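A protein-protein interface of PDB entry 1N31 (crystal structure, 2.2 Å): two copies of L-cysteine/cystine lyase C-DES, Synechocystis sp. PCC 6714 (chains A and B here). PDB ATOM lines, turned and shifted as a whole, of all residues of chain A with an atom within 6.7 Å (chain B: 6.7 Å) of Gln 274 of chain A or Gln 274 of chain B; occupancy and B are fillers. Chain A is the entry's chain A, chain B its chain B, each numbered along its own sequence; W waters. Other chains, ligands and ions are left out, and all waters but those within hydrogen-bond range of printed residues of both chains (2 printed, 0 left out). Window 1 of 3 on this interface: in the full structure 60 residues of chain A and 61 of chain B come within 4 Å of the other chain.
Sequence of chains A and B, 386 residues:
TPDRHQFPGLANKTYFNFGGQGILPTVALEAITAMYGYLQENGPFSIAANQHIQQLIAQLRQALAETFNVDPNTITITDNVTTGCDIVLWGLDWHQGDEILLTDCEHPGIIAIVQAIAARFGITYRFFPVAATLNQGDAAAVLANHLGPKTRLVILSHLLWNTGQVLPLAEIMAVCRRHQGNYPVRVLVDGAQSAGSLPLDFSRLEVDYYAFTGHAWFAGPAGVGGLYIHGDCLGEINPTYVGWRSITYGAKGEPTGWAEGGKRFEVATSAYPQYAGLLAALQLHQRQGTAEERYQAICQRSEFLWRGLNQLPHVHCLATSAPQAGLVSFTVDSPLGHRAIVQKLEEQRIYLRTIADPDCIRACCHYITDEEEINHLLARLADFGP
The side-chain amide nitrogen (NE2) of Gln 274 of chain B sits close to the side-chain amide nitrogen (NE2) of Gln 274 of chain A (2.6 Å). NE2 of Gln 274 of chain A lies within hydrogen-bond range of OH of Tyr 36 of chain B (2.5 Å). OH of Tyr 36 of chain A lies close to NE2 of Gln 274 of chain B (2.2 Å).
The side-chain amide oxygen of Gln 274 of chain B lies close to the backbone carbonyl oxygen of Ala 271 of chain B. The side-chain hydroxyl (OG) of Ser 270 of chain A lies close to the side-chain hydroxyl (OH) of Tyr 275 of chain A (3.3 Å). O of Ala 271 of chain A sits close to OE1 of Gln 274 of chain A (3.2 Å). The side-chain hydroxyl of Ser 270 of chain B sits close to the side-chain hydroxyl of Tyr 275 of chain B.
Among the printed residues, merely in contact across the chains: Ile 32 of chain A with Tyr 36 of chain B (3.6 Å), Tyr 36 of chain A with Ile 32 of chain B (3.5 Å), Ala 222 of chain A with Ser 270 of chain B (3.5 Å), Ala 222 of chain A with Ala 271 of chain B (3.3 Å), Gly 223 of chain A with Ser 270 of chain B (3.7 Å), Gly 223 of chain A with Ala 271 of chain B (3.7 Å), Ser 270 of chain A with Ala 222 of chain B (3.5 Å), Ser 270 of chain A with Gly 223 of chain B (3.7 Å), Ala 271 of chain A with Ala 222 of chain B (3.4 Å) and Ala 271 of chain A with Gly 223 of chain B (3.7 Å).
Gln 274 of chain A touches two residues of chain B. Of chain A, only Tyr 36 (2.2 Å) and Gln 274 (2.6 Å) come within 4 Å of Gln 274 of chain B. Of the printed residues of chain B, Gly 223 of chain A touches Ser 270 (3.7 Å) and Ala 271 (3.7 Å). Printed residues of chain B within 4 Å of Tyr 36 of chain A: Ile 32 (3.5 Å) and Gln 274 (2.2 Å). Of the printed residues of chain A, Ala 222 of chain B touches Ser 270 and Ala 271. Of the printed residues of chain B, Ile 32 of chain A touches Tyr 36 (3.6 Å). Tyr 275 of chain B touches none of the printed residues of chain A.
Of the 20 printed residues of chain B, 7 touch a printed residue of chain A. Hydrophobic or aromatic side chains of chain B within 4 Å of the printed part of chain A: Ile 32, Tyr 36, Ala 222 and Ala 271. Of the 21 printed residues of chain A, 7 touch a printed residue of chain B. Among the printed residues, no Asp or Glu carboxylate lies within 4 Å of a Lys or Arg side-chain nitrogen of the other chain.
Tyr 36 of chain A touches Gln 274 of chain B, and with the chains exchanged Gln 274 of chain A touches Tyr 36 of chain B. Gly 223 of chain A touches Ala 271 of chain B, and with the chains exchanged Ala 271 of chain A touches Gly 223 of chain B. Gln 274 of chain B touches its own counterpart, Gln 274 of chain A.
Water W2 lies within hydrogen-bond range of O of Ala 222 of chain A (2.6 Å) and OH of Tyr 36 of chain B (3.1 Å). Water W1 lies within hydrogen-bond range of N of Ala 271 of chain B and O of Gly 223 of chain A.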
ATOM      1  N   ALA A  31      22.543  22.818 -35.021  1.00  0.00           N
ATOM      2  CA  ALA A  31      21.232  22.415 -34.524  1.00  0.00           C
ATOM      3  C   ALA A  31      21.333  21.682 -33.175  1.00  0.00           C
ATOM      4  O   ALA A  31      20.459  21.826 -32.318  1.00  0.00           O
ATOM      5  CB  ALA A  31      20.531  21.528 -35.545  1.00  0.00           C
ATOM      6  N   ILE A  32      22.396  20.904 -32.991  1.00  0.00           N
ATOM      7  CA  ILE A  32      22.609  20.174 -31.742  1.00  0.00           C
ATOM      8  C   ILE A  32      22.874  21.166 -30.608  1.00  0.00           C
ATOM      9  O   ILE A  32      22.244  21.105 -29.543  1.00  0.00           O
ATOM     10  CB  ILE A  32      23.805  19.189 -31.867  1.00  0.00           C
ATOM     11  CG1 ILE A  32      23.377  17.984 -32.721  1.00  0.00           C
ATOM     12  CG2 ILE A  32      24.290  18.768 -30.470  1.00  0.00           C
ATOM     13  CD1 ILE A  32      24.511  17.116 -33.216  1.00  0.00           C
ATOM     14  N   MET A  35      19.789  23.221 -29.661  1.00  0.00           N
ATOM     15  CA  MET A  35      18.799  22.477 -28.867  1.00  0.00           C
ATOM     16  C   MET A  35      19.156  22.449 -27.386  1.00  0.00           C
ATOM     17  O   MET A  35      18.281  22.527 -26.523  1.00  0.00           O
ATOM     18  CB  MET A  35      18.640  21.039 -29.396  1.00  0.00           C
ATOM     19  CG  MET A  35      17.563  20.204 -28.686  1.00  0.00           C
ATOM     20  SD  MET A  35      15.857  20.766 -28.836  1.00  0.00           S
ATOM     21  CE  MET A  35      15.834  21.319 -30.610  1.00  0.00           C
ATOM     22  N   TYR A  36      20.442  22.314 -27.088  1.00  0.00           N
ATOM     23  CA  TYR A  36      20.884  22.334 -25.686  1.00  0.00           C
ATOM     24  C   TYR A  36      20.591  23.703 -25.083  1.00  0.00           C
ATOM     25  O   TYR A  36      20.212  23.796 -23.913  1.00  0.00           O
ATOM     26  CB  TYR A  36      22.383  22.072 -25.587  1.00  0.00           C
ATOM     27  CG  TYR A  36      22.739  20.617 -25.631  1.00  0.00           C
ATOM     28  CD1 TYR A  36      23.555  20.120 -26.633  1.00  0.00           C
ATOM     29  CD2 TYR A  36      22.274  19.734 -24.652  1.00  0.00           C
ATOM     30  CE1 TYR A  36      23.906  18.795 -26.673  1.00  0.00           C
ATOM     31  CE2 TYR A  36      22.624  18.386 -24.681  1.00  0.00           C
ATOM     32  CZ  TYR A  36      23.444  17.930 -25.699  1.00  0.00           C
ATOM     33  OH  TYR A  36      23.863  16.630 -25.789  1.00  0.00           O
ATOM     34  N   LEU A  56       9.873  18.654 -32.351  1.00  0.00           N
ATOM     35  CA  LEU A  56      11.113  18.245 -33.004  1.00  0.00           C
ATOM     36  C   LEU A  56      10.985  16.798 -33.489  1.00  0.00           C
ATOM     37  O   LEU A  56      11.319  16.486 -34.633  1.00  0.00           O
ATOM     38  CB  LEU A  56      12.313  18.362 -32.043  1.00  0.00           C
ATOM     39  CG  LEU A  56      13.608  17.696 -32.525  1.00  0.00           C
ATOM     40  CD1 LEU A  56      14.086  18.373 -33.802  1.00  0.00           C
ATOM     41  CD2 LEU A  56      14.668  17.792 -31.452  1.00  0.00           C
ATOM     42  N   LEU A  60      11.292  15.358 -37.438  1.00  0.00           N
ATOM     43  CA  LEU A  60      12.252  14.379 -37.923  1.00  0.00           C
ATOM     44  C   LEU A  60      11.499  13.185 -38.533  1.00  0.00           C
ATOM     45  O   LEU A  60      11.896  12.676 -39.581  1.00  0.00           O
ATOM     46  CB  LEU A  60      13.180  13.913 -36.790  1.00  0.00           C
ATOM     47  CG  LEU A  60      14.155  12.761 -37.105  1.00  0.00           C
ATOM     48  CD1 LEU A  60      15.068  13.137 -38.272  1.00  0.00           C
ATOM     49  CD2 LEU A  60      15.016  12.419 -35.861  1.00  0.00           C
ATOM     50  N   GLY A 220      24.443  12.155 -40.204  1.00  0.00           N
ATOM     51  CA  GLY A 220      23.923  12.696 -38.959  1.00  0.00           C
ATOM     52  C   GLY A 220      24.866  12.303 -37.817  1.00  0.00           C
ATOM     53  O   GLY A 220      25.867  11.633 -38.054  1.00  0.00           O
ATOM     54  N   PRO A 221      24.585  12.694 -36.566  1.00  0.00           N
ATOM     55  CA  PRO A 221      25.455  12.342 -35.435  1.00  0.00           C
ATOM     56  C   PRO A 221      25.209  10.901 -34.996  1.00  0.00           C
ATOM     57  O   PRO A 221      24.139  10.366 -35.261  1.00  0.00           O
ATOM     58  CB  PRO A 221      25.037  13.347 -34.340  1.00  0.00           C
ATOM     59  CG  PRO A 221      23.591  13.539 -34.597  1.00  0.00           C
ATOM     60  CD  PRO A 221      23.499  13.591 -36.140  1.00  0.00           C
ATOM     61  N   ALA A 222      26.198  10.281 -34.342  1.00  0.00           N
ATOM     62  CA  ALA A 222      26.021   8.919 -33.852  1.00  0.00           C
ATOM     63  C   ALA A 222      24.900   8.938 -32.806  1.00  0.00           C
ATOM     64  O   ALA A 222      24.830   9.859 -31.997  1.00  0.00           O
ATOM     65  CB  ALA A 222      27.313   8.394 -33.225  1.00  0.00           C
ATOM     66  N   GLY A 223      24.025   7.930 -32.843  1.00  0.00           N
ATOM     67  CA  GLY A 223      22.934   7.839 -31.887  1.00  0.00           C
ATOM     68  C   GLY A 223      21.494   8.005 -32.370  1.00  0.00           C
ATOM     69  O   GLY A 223      20.556   7.956 -31.574  1.00  0.00           O
ATOM     70  N   VAL A 224      21.284   8.217 -33.661  1.00  0.00           N
ATOM     71  CA  VAL A 224      19.920   8.368 -34.158  1.00  0.00           C
ATOM     72  C   VAL A 224      19.745   7.560 -35.437  1.00  0.00           C
ATOM     73  O   VAL A 224      20.563   7.646 -36.355  1.00  0.00           O
ATOM     74  CB  VAL A 224      19.575   9.847 -34.464  1.00  0.00           C
ATOM     75  CG1 VAL A 224      18.054   9.977 -34.721  1.00  0.00           C
ATOM     76  CG2 VAL A 224      19.976  10.742 -33.310  1.00  0.00           C
ATOM     77  N   SER A 270      15.296  10.110 -24.863  1.00  0.00           N
ATOM     78  CA  SER A 270      16.370   9.997 -25.857  1.00  0.00           C
ATOM     79  C   SER A 270      17.205  11.274 -25.980  1.00  0.00           C
ATOM     80  O   SER A 270      16.879  12.314 -25.401  1.00  0.00           O
ATOM     81  CB  SER A 270      15.782   9.656 -27.228  1.00  0.00           C
ATOM     82  OG  SER A 270      15.282   8.338 -27.252  1.00  0.00           O
ATOM     83  N   ALA A 271      18.277  11.190 -26.761  1.00  0.00           N
ATOM     84  CA  ALA A 271      19.149  12.333 -26.963  1.00  0.00           C
ATOM     85  C   ALA A 271      18.524  13.262 -28.011  1.00  0.00           C
ATOM     86  O   ALA A 271      18.961  13.299 -29.158  1.00  0.00           O
ATOM     87  CB  ALA A 271      20.515  11.854 -27.424  1.00  0.00           C
ATOM     88  N   TYR A 272      17.510  14.012 -27.594  1.00  0.00           N
ATOM     89  CA  TYR A 272      16.771  14.921 -28.470  1.00  0.00           C
ATOM     90  C   TYR A 272      17.623  15.872 -29.277  1.00  0.00           C
ATOM     91  O   TYR A 272      17.375  16.066 -30.455  1.00  0.00           O
ATOM     92  CB  TYR A 272      15.745  15.711 -27.645  1.00  0.00           C
ATOM     93  CG  TYR A 272      14.878  14.819 -26.784  1.00  0.00           C
ATOM     94  CD1 TYR A 272      14.698  15.087 -25.429  1.00  0.00           C
ATOM     95  CD2 TYR A 272      14.249  13.693 -27.323  1.00  0.00           C
ATOM     96  CE1 TYR A 272      13.919  14.255 -24.634  1.00  0.00           C
ATOM     97  CE2 TYR A 272      13.460  12.859 -26.526  1.00  0.00           C
ATOM     98  CZ  TYR A 272      13.303  13.145 -25.191  1.00  0.00           C
ATOM     99  OH  TYR A 272      12.524  12.334 -24.407  1.00  0.00           O
ATOM    100  N   PRO A 273      18.647  16.483 -28.659  1.00  0.00           N
ATOM    101  CA  PRO A 273      19.452  17.401 -29.477  1.00  0.00           C
ATOM    102  C   PRO A 273      20.072  16.689 -30.692  1.00  0.00           C
ATOM    103  O   PRO A 273      20.308  17.305 -31.736  1.00  0.00           O
ATOM    104  CB  PRO A 273      20.501  17.922 -28.494  1.00  0.00           C
ATOM    105  CG  PRO A 273      19.791  17.754 -27.113  1.00  0.00           C
ATOM    106  CD  PRO A 273      19.158  16.405 -27.277  1.00  0.00           C
ATOM    107  N   GLN A 274      20.360  15.400 -30.557  1.00  0.00           N
ATOM    108  CA  GLN A 274      20.920  14.652 -31.694  1.00  0.00           C
ATOM    109  C   GLN A 274      19.875  14.528 -32.817  1.00  0.00           C
ATOM    110  O   GLN A 274      20.221  14.458 -33.996  1.00  0.00           O
ATOM    111  CB  GLN A 274      21.371  13.246 -31.274  1.00  0.00           C
ATOM    112  CG  GLN A 274      22.782  13.186 -30.700  1.00  0.00           C
ATOM    113  CD  GLN A 274      22.919  14.045 -29.462  1.00  0.00           C
ATOM    114  OE1 GLN A 274      22.014  14.079 -28.606  1.00  0.00           O
ATOM    115  NE2 GLN A 274      24.052  14.748 -29.348  1.00  0.00           N
ATOM    116  N   TYR A 275      18.603  14.459 -32.423  1.00  0.00           N
ATOM    117  CA  TYR A 275      17.516  14.376 -33.386  1.00  0.00           C
ATOM    118  C   TYR A 275      17.560  15.621 -34.287  1.00  0.00           C
ATOM    119  O   TYR A 275      17.440  15.532 -35.514  1.00  0.00           O
ATOM    120  CB  TYR A 275      16.167  14.350 -32.669  1.00  0.00           C
ATOM    121  CG  TYR A 275      15.759  13.033 -32.058  1.00  0.00           C
ATOM    122  CD1 TYR A 275      14.452  12.843 -31.621  1.00  0.00           C
ATOM    123  CD2 TYR A 275      16.658  11.986 -31.907  1.00  0.00           C
ATOM    124  CE1 TYR A 275      14.048  11.651 -31.048  1.00  0.00           C
ATOM    125  CE2 TYR A 275      16.265  10.773 -31.326  1.00  0.00           C
ATOM    126  CZ  TYR A 275      14.956  10.616 -30.899  1.00  0.00           C
ATOM    127  OH  TYR A 275      14.540   9.446 -30.316  1.00  0.00           O
ATOM    128  N   ALA A 276      17.738  16.778 -33.658  1.00  0.00           N
ATOM    129  CA  ALA A 276      17.780  18.043 -34.379  1.00  0.00           C
ATOM    130  C   ALA A 276      18.972  18.014 -35.325  1.00  0.00           C
ATOM    131  O   ALA A 276      18.937  18.603 -36.400  1.00  0.00           O
ATOM    132  CB  ALA A 276      17.906  19.207 -33.383  1.00  0.00           C
ATOM    133  N   GLY A 277      20.029  17.317 -34.915  1.00  0.00           N
ATOM    134  CA  GLY A 277      21.212  17.216 -35.754  1.00  0.00           C
ATOM    135  C   GLY A 277      20.932  16.427 -37.027  1.00  0.00           C
ATOM    136  O   GLY A 277      21.301  16.846 -38.122  1.00  0.00           O
ATOM    137  N   LEU A 278      20.287  15.275 -36.884  1.00  0.00           N
ATOM    138  CA  LEU A 278      19.946  14.439 -38.034  1.00  0.00           C
ATOM    139  C   LEU A 278      18.989  15.203 -38.995  1.00  0.00           C
ATOM    140  O   LEU A 278      19.136  15.163 -40.215  1.00  0.00           O
ATOM    141  CB  LEU A 278      19.277  13.140 -37.556  1.00  0.00           C
ATOM    142  CG  LEU A 278      18.735  12.239 -38.697  1.00  0.00           C
ATOM    143  CD1 LEU A 278      19.875  11.893 -39.662  1.00  0.00           C
ATOM    144  CD2 LEU A 278      18.119  10.940 -38.115  1.00  0.00           C
ATOM    145  N   LEU A 279      18.003  15.891 -38.429  1.00  0.00           N
ATOM    146  CA  LEU A 279      17.060  16.661 -39.229  1.00  0.00           C
ATOM    147  C   LEU A 279      17.843  17.658 -40.106  1.00  0.00           C
ATOM    148  O   LEU A 279      17.607  17.775 -41.300  1.00  0.00           O
ATOM    149  CB  LEU A 279      16.124  17.436 -38.311  1.00  0.00           C
ATOM    150  CG  LEU A 279      14.663  17.634 -38.708  1.00  0.00           C
ATOM    151  CD1 LEU A 279      14.110  18.899 -37.988  1.00  0.00           C
ATOM    152  CD2 LEU A 279      14.531  17.763 -40.195  1.00  0.00           C
ATOM    153  N   ILE B  32      30.685  17.429 -23.887  1.00  0.00           N
ATOM    154  CA  ILE B  32      29.914  17.021 -25.067  1.00  0.00           C
ATOM    155  C   ILE B  32      30.518  17.696 -26.323  1.00  0.00           C
ATOM    156  O   ILE B  32      30.881  17.040 -27.300  1.00  0.00           O
ATOM    157  CB  ILE B  32      28.415  17.426 -24.910  1.00  0.00           C
ATOM    158  CG1 ILE B  32      27.751  16.525 -23.846  1.00  0.00           C
ATOM    159  CG2 ILE B  32      27.691  17.346 -26.253  1.00  0.00           C
ATOM    160  CD1 ILE B  32      26.370  16.970 -23.392  1.00  0.00           C
ATOM    161  N   MET B  35      33.903  16.343 -27.312  1.00  0.00           N
ATOM    162  CA  MET B  35      33.854  15.024 -27.945  1.00  0.00           C
ATOM    163  C   MET B  35      33.554  15.103 -29.431  1.00  0.00           C
ATOM    164  O   MET B  35      34.088  14.318 -30.196  1.00  0.00           O
ATOM    165  CB  MET B  35      32.817  14.119 -27.267  1.00  0.00           C
ATOM    166  CG  MET B  35      32.836  12.659 -27.760  1.00  0.00           C
ATOM    167  SD  MET B  35      34.495  11.858 -27.575  1.00  0.00           S
ATOM    168  CE  MET B  35      34.838  12.149 -25.862  1.00  0.00           C
ATOM    169  N   TYR B  36      32.677  16.028 -29.824  1.00  0.00           N
ATOM    170  CA  TYR B  36      32.326  16.233 -31.235  1.00  0.00           C
ATOM    171  C   TYR B  36      33.550  16.740 -31.968  1.00  0.00           C
ATOM    172  O   TYR B  36      33.823  16.338 -33.093  1.00  0.00           O
ATOM    173  CB  TYR B  36      31.194  17.250 -31.377  1.00  0.00           C
ATOM    174  CG  TYR B  36      29.840  16.637 -31.204  1.00  0.00           C
ATOM    175  CD1 TYR B  36      28.992  17.054 -30.180  1.00  0.00           C
ATOM    176  CD2 TYR B  36      29.400  15.633 -32.066  1.00  0.00           C
ATOM    177  CE1 TYR B  36      27.739  16.490 -30.018  1.00  0.00           C
ATOM    178  CE2 TYR B  36      28.151  15.065 -31.914  1.00  0.00           C
ATOM    179  CZ  TYR B  36      27.326  15.494 -30.892  1.00  0.00           C
ATOM    180  OH  TYR B  36      26.083  14.939 -30.767  1.00  0.00           O
ATOM    181  N   LEU B  56      36.259   6.016 -23.548  1.00  0.00           N
ATOM    182  CA  LEU B  56      35.230   6.829 -22.903  1.00  0.00           C
ATOM    183  C   LEU B  56      34.168   5.938 -22.252  1.00  0.00           C
ATOM    184  O   LEU B  56      33.763   6.173 -21.115  1.00  0.00           O
ATOM    185  CB  LEU B  56      34.554   7.773 -23.904  1.00  0.00           C
ATOM    186  CG  LEU B  56      33.282   8.454 -23.392  1.00  0.00           C
ATOM    187  CD1 LEU B  56      33.592   9.402 -22.241  1.00  0.00           C
ATOM    188  CD2 LEU B  56      32.640   9.204 -24.549  1.00  0.00           C
ATOM    189  N   LEU B  60      33.085   5.877 -18.196  1.00  0.00           N
ATOM    190  CA  LEU B  60      31.737   6.106 -17.672  1.00  0.00           C
ATOM    191  C   LEU B  60      31.263   4.862 -16.865  1.00  0.00           C
ATOM    192  O   LEU B  60      30.683   4.996 -15.788  1.00  0.00           O
ATOM    193  CB  LEU B  60      30.752   6.396 -18.822  1.00  0.00           C
ATOM    194  CG  LEU B  60      29.275   6.529 -18.410  1.00  0.00           C
ATOM    195  CD1 LEU B  60      29.162   7.668 -17.357  1.00  0.00           C
ATOM    196  CD2 LEU B  60      28.393   6.817 -19.626  1.00  0.00           C
ATOM    197  N   GLY B 220      22.854  14.867 -15.877  1.00  0.00           N
ATOM    198  CA  GLY B 220      23.550  14.619 -17.129  1.00  0.00           C
ATOM    199  C   GLY B 220      22.585  14.990 -18.268  1.00  0.00           C
ATOM    200  O   GLY B 220      21.468  15.427 -18.008  1.00  0.00           O
ATOM    201  N   PRO B 221      22.977  14.825 -19.537  1.00  0.00           N
ATOM    202  CA  PRO B 221      22.108  15.160 -20.668  1.00  0.00           C
ATOM    203  C   PRO B 221      21.054  14.079 -20.920  1.00  0.00           C
ATOM    204  O   PRO B 221      21.266  12.928 -20.540  1.00  0.00           O
ATOM    205  CB  PRO B 221      23.094  15.264 -21.821  1.00  0.00           C
ATOM    206  CG  PRO B 221      24.058  14.186 -21.514  1.00  0.00           C
ATOM    207  CD  PRO B 221      24.290  14.348 -20.007  1.00  0.00           C
ATOM    208  N   ALA B 222      19.932  14.438 -21.551  1.00  0.00           N
ATOM    209  CA  ALA B 222      18.886  13.453 -21.885  1.00  0.00           C
ATOM    210  C   ALA B 222      19.472  12.427 -22.852  1.00  0.00           C
ATOM    211  O   ALA B 222      20.175  12.787 -23.799  1.00  0.00           O
ATOM    212  CB  ALA B 222      17.700  14.136 -22.537  1.00  0.00           C
ATOM    213  N   GLY B 223      19.227  11.149 -22.595  1.00  0.00           N
ATOM    214  CA  GLY B 223      19.749  10.119 -23.490  1.00  0.00           C
ATOM    215  C   GLY B 223      20.758   9.114 -22.942  1.00  0.00           C
ATOM    216  O   GLY B 223      21.200   8.225 -23.664  1.00  0.00           O
ATOM    217  N   VAL B 224      21.141   9.234 -21.680  1.00  0.00           N
ATOM    218  CA  VAL B 224      22.108   8.283 -21.120  1.00  0.00           C
ATOM    219  C   VAL B 224      21.646   7.812 -19.736  1.00  0.00           C
ATOM    220  O   VAL B 224      21.333   8.634 -18.863  1.00  0.00           O
ATOM    221  CB  VAL B 224      23.503   8.906 -21.004  1.00  0.00           C
ATOM    222  CG1 VAL B 224      24.541   7.817 -20.678  1.00  0.00           C
ATOM    223  CG2 VAL B 224      23.877   9.587 -22.299  1.00  0.00           C
ATOM    224  N   SER B 270      25.697   4.484 -30.238  1.00  0.00           N
ATOM    225  CA  SER B 270      24.999   5.383 -29.329  1.00  0.00           C
ATOM    226  C   SER B 270      25.566   6.804 -29.432  1.00  0.00           C
ATOM    227  O   SER B 270      26.573   7.023 -30.100  1.00  0.00           O
ATOM    228  CB  SER B 270      25.122   4.877 -27.882  1.00  0.00           C
ATOM    229  OG  SER B 270      24.348   3.706 -27.681  1.00  0.00           O
ATOM    230  N   ALA B 271      24.927   7.765 -28.772  1.00  0.00           N
ATOM    231  CA  ALA B 271      25.397   9.155 -28.811  1.00  0.00           C
ATOM    232  C   ALA B 271      26.578   9.331 -27.845  1.00  0.00           C
ATOM    233  O   ALA B 271      26.438   9.886 -26.761  1.00  0.00           O
ATOM    234  CB  ALA B 271      24.257  10.072 -28.439  1.00  0.00           C
ATOM    235  N   TYR B 272      27.746   8.854 -28.255  1.00  0.00           N
ATOM    236  CA  TYR B 272      28.946   8.893 -27.401  1.00  0.00           C
ATOM    237  C   TYR B 272      29.244  10.216 -26.729  1.00  0.00           C
ATOM    238  O   TYR B 272      29.586  10.255 -25.548  1.00  0.00           O
ATOM    239  CB  TYR B 272      30.160   8.425 -28.211  1.00  0.00           C
ATOM    240  CG  TYR B 272      29.884   7.108 -28.892  1.00  0.00           C
ATOM    241  CD1 TYR B 272      30.091   6.953 -30.264  1.00  0.00           C
ATOM    242  CD2 TYR B 272      29.410   6.004 -28.160  1.00  0.00           C
ATOM    243  CE1 TYR B 272      29.839   5.737 -30.900  1.00  0.00           C
ATOM    244  CE2 TYR B 272      29.154   4.788 -28.784  1.00  0.00           C
ATOM    245  CZ  TYR B 272      29.374   4.660 -30.156  1.00  0.00           C
ATOM    246  OH  TYR B 272      29.164   3.442 -30.766  1.00  0.00           O
ATOM    247  N   PRO B 273      29.118  11.323 -27.473  1.00  0.00           N
ATOM    248  CA  PRO B 273      29.400  12.613 -26.839  1.00  0.00           C
ATOM    249  C   PRO B 273      28.546  12.823 -25.595  1.00  0.00           C
ATOM    250  O   PRO B 273      28.984  13.502 -24.659  1.00  0.00           O
ATOM    251  CB  PRO B 273      29.094  13.631 -27.946  1.00  0.00           C
ATOM    252  CG  PRO B 273      29.357  12.830 -29.225  1.00  0.00           C
ATOM    253  CD  PRO B 273      28.747  11.482 -28.891  1.00  0.00           C
ATOM    254  N   GLN B 274      27.342  12.246 -25.574  1.00  0.00           N
ATOM    255  CA  GLN B 274      26.476  12.398 -24.398  1.00  0.00           C
ATOM    256  C   GLN B 274      27.090  11.649 -23.208  1.00  0.00           C
ATOM    257  O   GLN B 274      26.905  12.036 -22.068  1.00  0.00           O
ATOM    258  CB  GLN B 274      25.045  11.872 -24.660  1.00  0.00           C
ATOM    259  CG  GLN B 274      24.073  12.916 -25.245  1.00  0.00           C
ATOM    260  CD  GLN B 274      24.583  13.426 -26.553  1.00  0.00           C
ATOM    261  OE1 GLN B 274      25.109  12.651 -27.359  1.00  0.00           O
ATOM    262  NE2 GLN B 274      24.439  14.729 -26.791  1.00  0.00           N
ATOM    263  N   TYR B 275      27.807  10.569 -23.495  1.00  0.00           N
ATOM    264  CA  TYR B 275      28.433   9.775 -22.456  1.00  0.00           C
ATOM    265  C   TYR B 275      29.448  10.658 -21.733  1.00  0.00           C
ATOM    266  O   TYR B 275      29.526  10.672 -20.499  1.00  0.00           O
ATOM    267  CB  TYR B 275      29.150   8.563 -23.060  1.00  0.00           C
ATOM    268  CG  TYR B 275      28.268   7.404 -23.502  1.00  0.00           C
ATOM    269  CD1 TYR B 275      28.828   6.165 -23.786  1.00  0.00           C
ATOM    270  CD2 TYR B 275      26.890   7.536 -23.638  1.00  0.00           C
ATOM    271  CE1 TYR B 275      28.050   5.091 -24.188  1.00  0.00           C
ATOM    272  CE2 TYR B 275      26.100   6.454 -24.047  1.00  0.00           C
ATOM    273  CZ  TYR B 275      26.694   5.238 -24.317  1.00  0.00           C
ATOM    274  OH  TYR B 275      25.955   4.155 -24.702  1.00  0.00           O
ATOM    275  N   ALA B 276      30.236  11.399 -22.505  1.00  0.00           N
ATOM    276  CA  ALA B 276      31.234  12.298 -21.914  1.00  0.00           C
ATOM    277  C   ALA B 276      30.534  13.351 -21.061  1.00  0.00           C
ATOM    278  O   ALA B 276      31.075  13.806 -20.061  1.00  0.00           O
ATOM    279  CB  ALA B 276      32.061  12.969 -23.020  1.00  0.00           C
ATOM    280  N   GLY B 277      29.332  13.746 -21.469  1.00  0.00           N
ATOM    281  CA  GLY B 277      28.581  14.708 -20.692  1.00  0.00           C
ATOM    282  C   GLY B 277      28.200  14.137 -19.323  1.00  0.00           C
ATOM    283  O   GLY B 277      28.407  14.792 -18.308  1.00  0.00           O
ATOM    284  N   LEU B 278      27.647  12.929 -19.280  1.00  0.00           N
ATOM    285  CA  LEU B 278      27.260  12.332 -18.008  1.00  0.00           C
ATOM    286  C   LEU B 278      28.485  12.117 -17.095  1.00  0.00           C
ATOM    287  O   LEU B 278      28.411  12.325 -15.892  1.00  0.00           O
ATOM    288  CB  LEU B 278      26.543  10.996 -18.244  1.00  0.00           C
ATOM    289  CG  LEU B 278      26.203  10.157 -16.991  1.00  0.00           C
ATOM    290  CD1 LEU B 278      25.316  10.952 -16.049  1.00  0.00           C
ATOM    291  CD2 LEU B 278      25.503   8.858 -17.398  1.00  0.00           C
ATOM    292  N   LEU B 279      29.602  11.694 -17.675  1.00  0.00           N
ATOM    293  CA  LEU B 279      30.822  11.477 -16.918  1.00  0.00           C
ATOM    294  C   LEU B 279      31.192  12.789 -16.198  1.00  0.00           C
ATOM    295  O   LEU B 279      31.445  12.797 -14.997  1.00  0.00           O
ATOM    296  CB  LEU B 279      31.957  11.081 -17.861  1.00  0.00           C
ATOM    297  CG  LEU B 279      33.025  10.066 -17.413  1.00  0.00           C
ATOM    298  CD1 LEU B 279      34.322  10.287 -18.223  1.00  0.00           C
ATOM    299  CD2 LEU B 279      33.308  10.184 -15.934  1.00  0.00           C
HETATM  300  O   HOH W   1      21.705   7.148 -28.424  1.00  0.00           O
HETATM  301  O   HOH W   2      26.412  11.912 -31.453  1.00  0.00           O
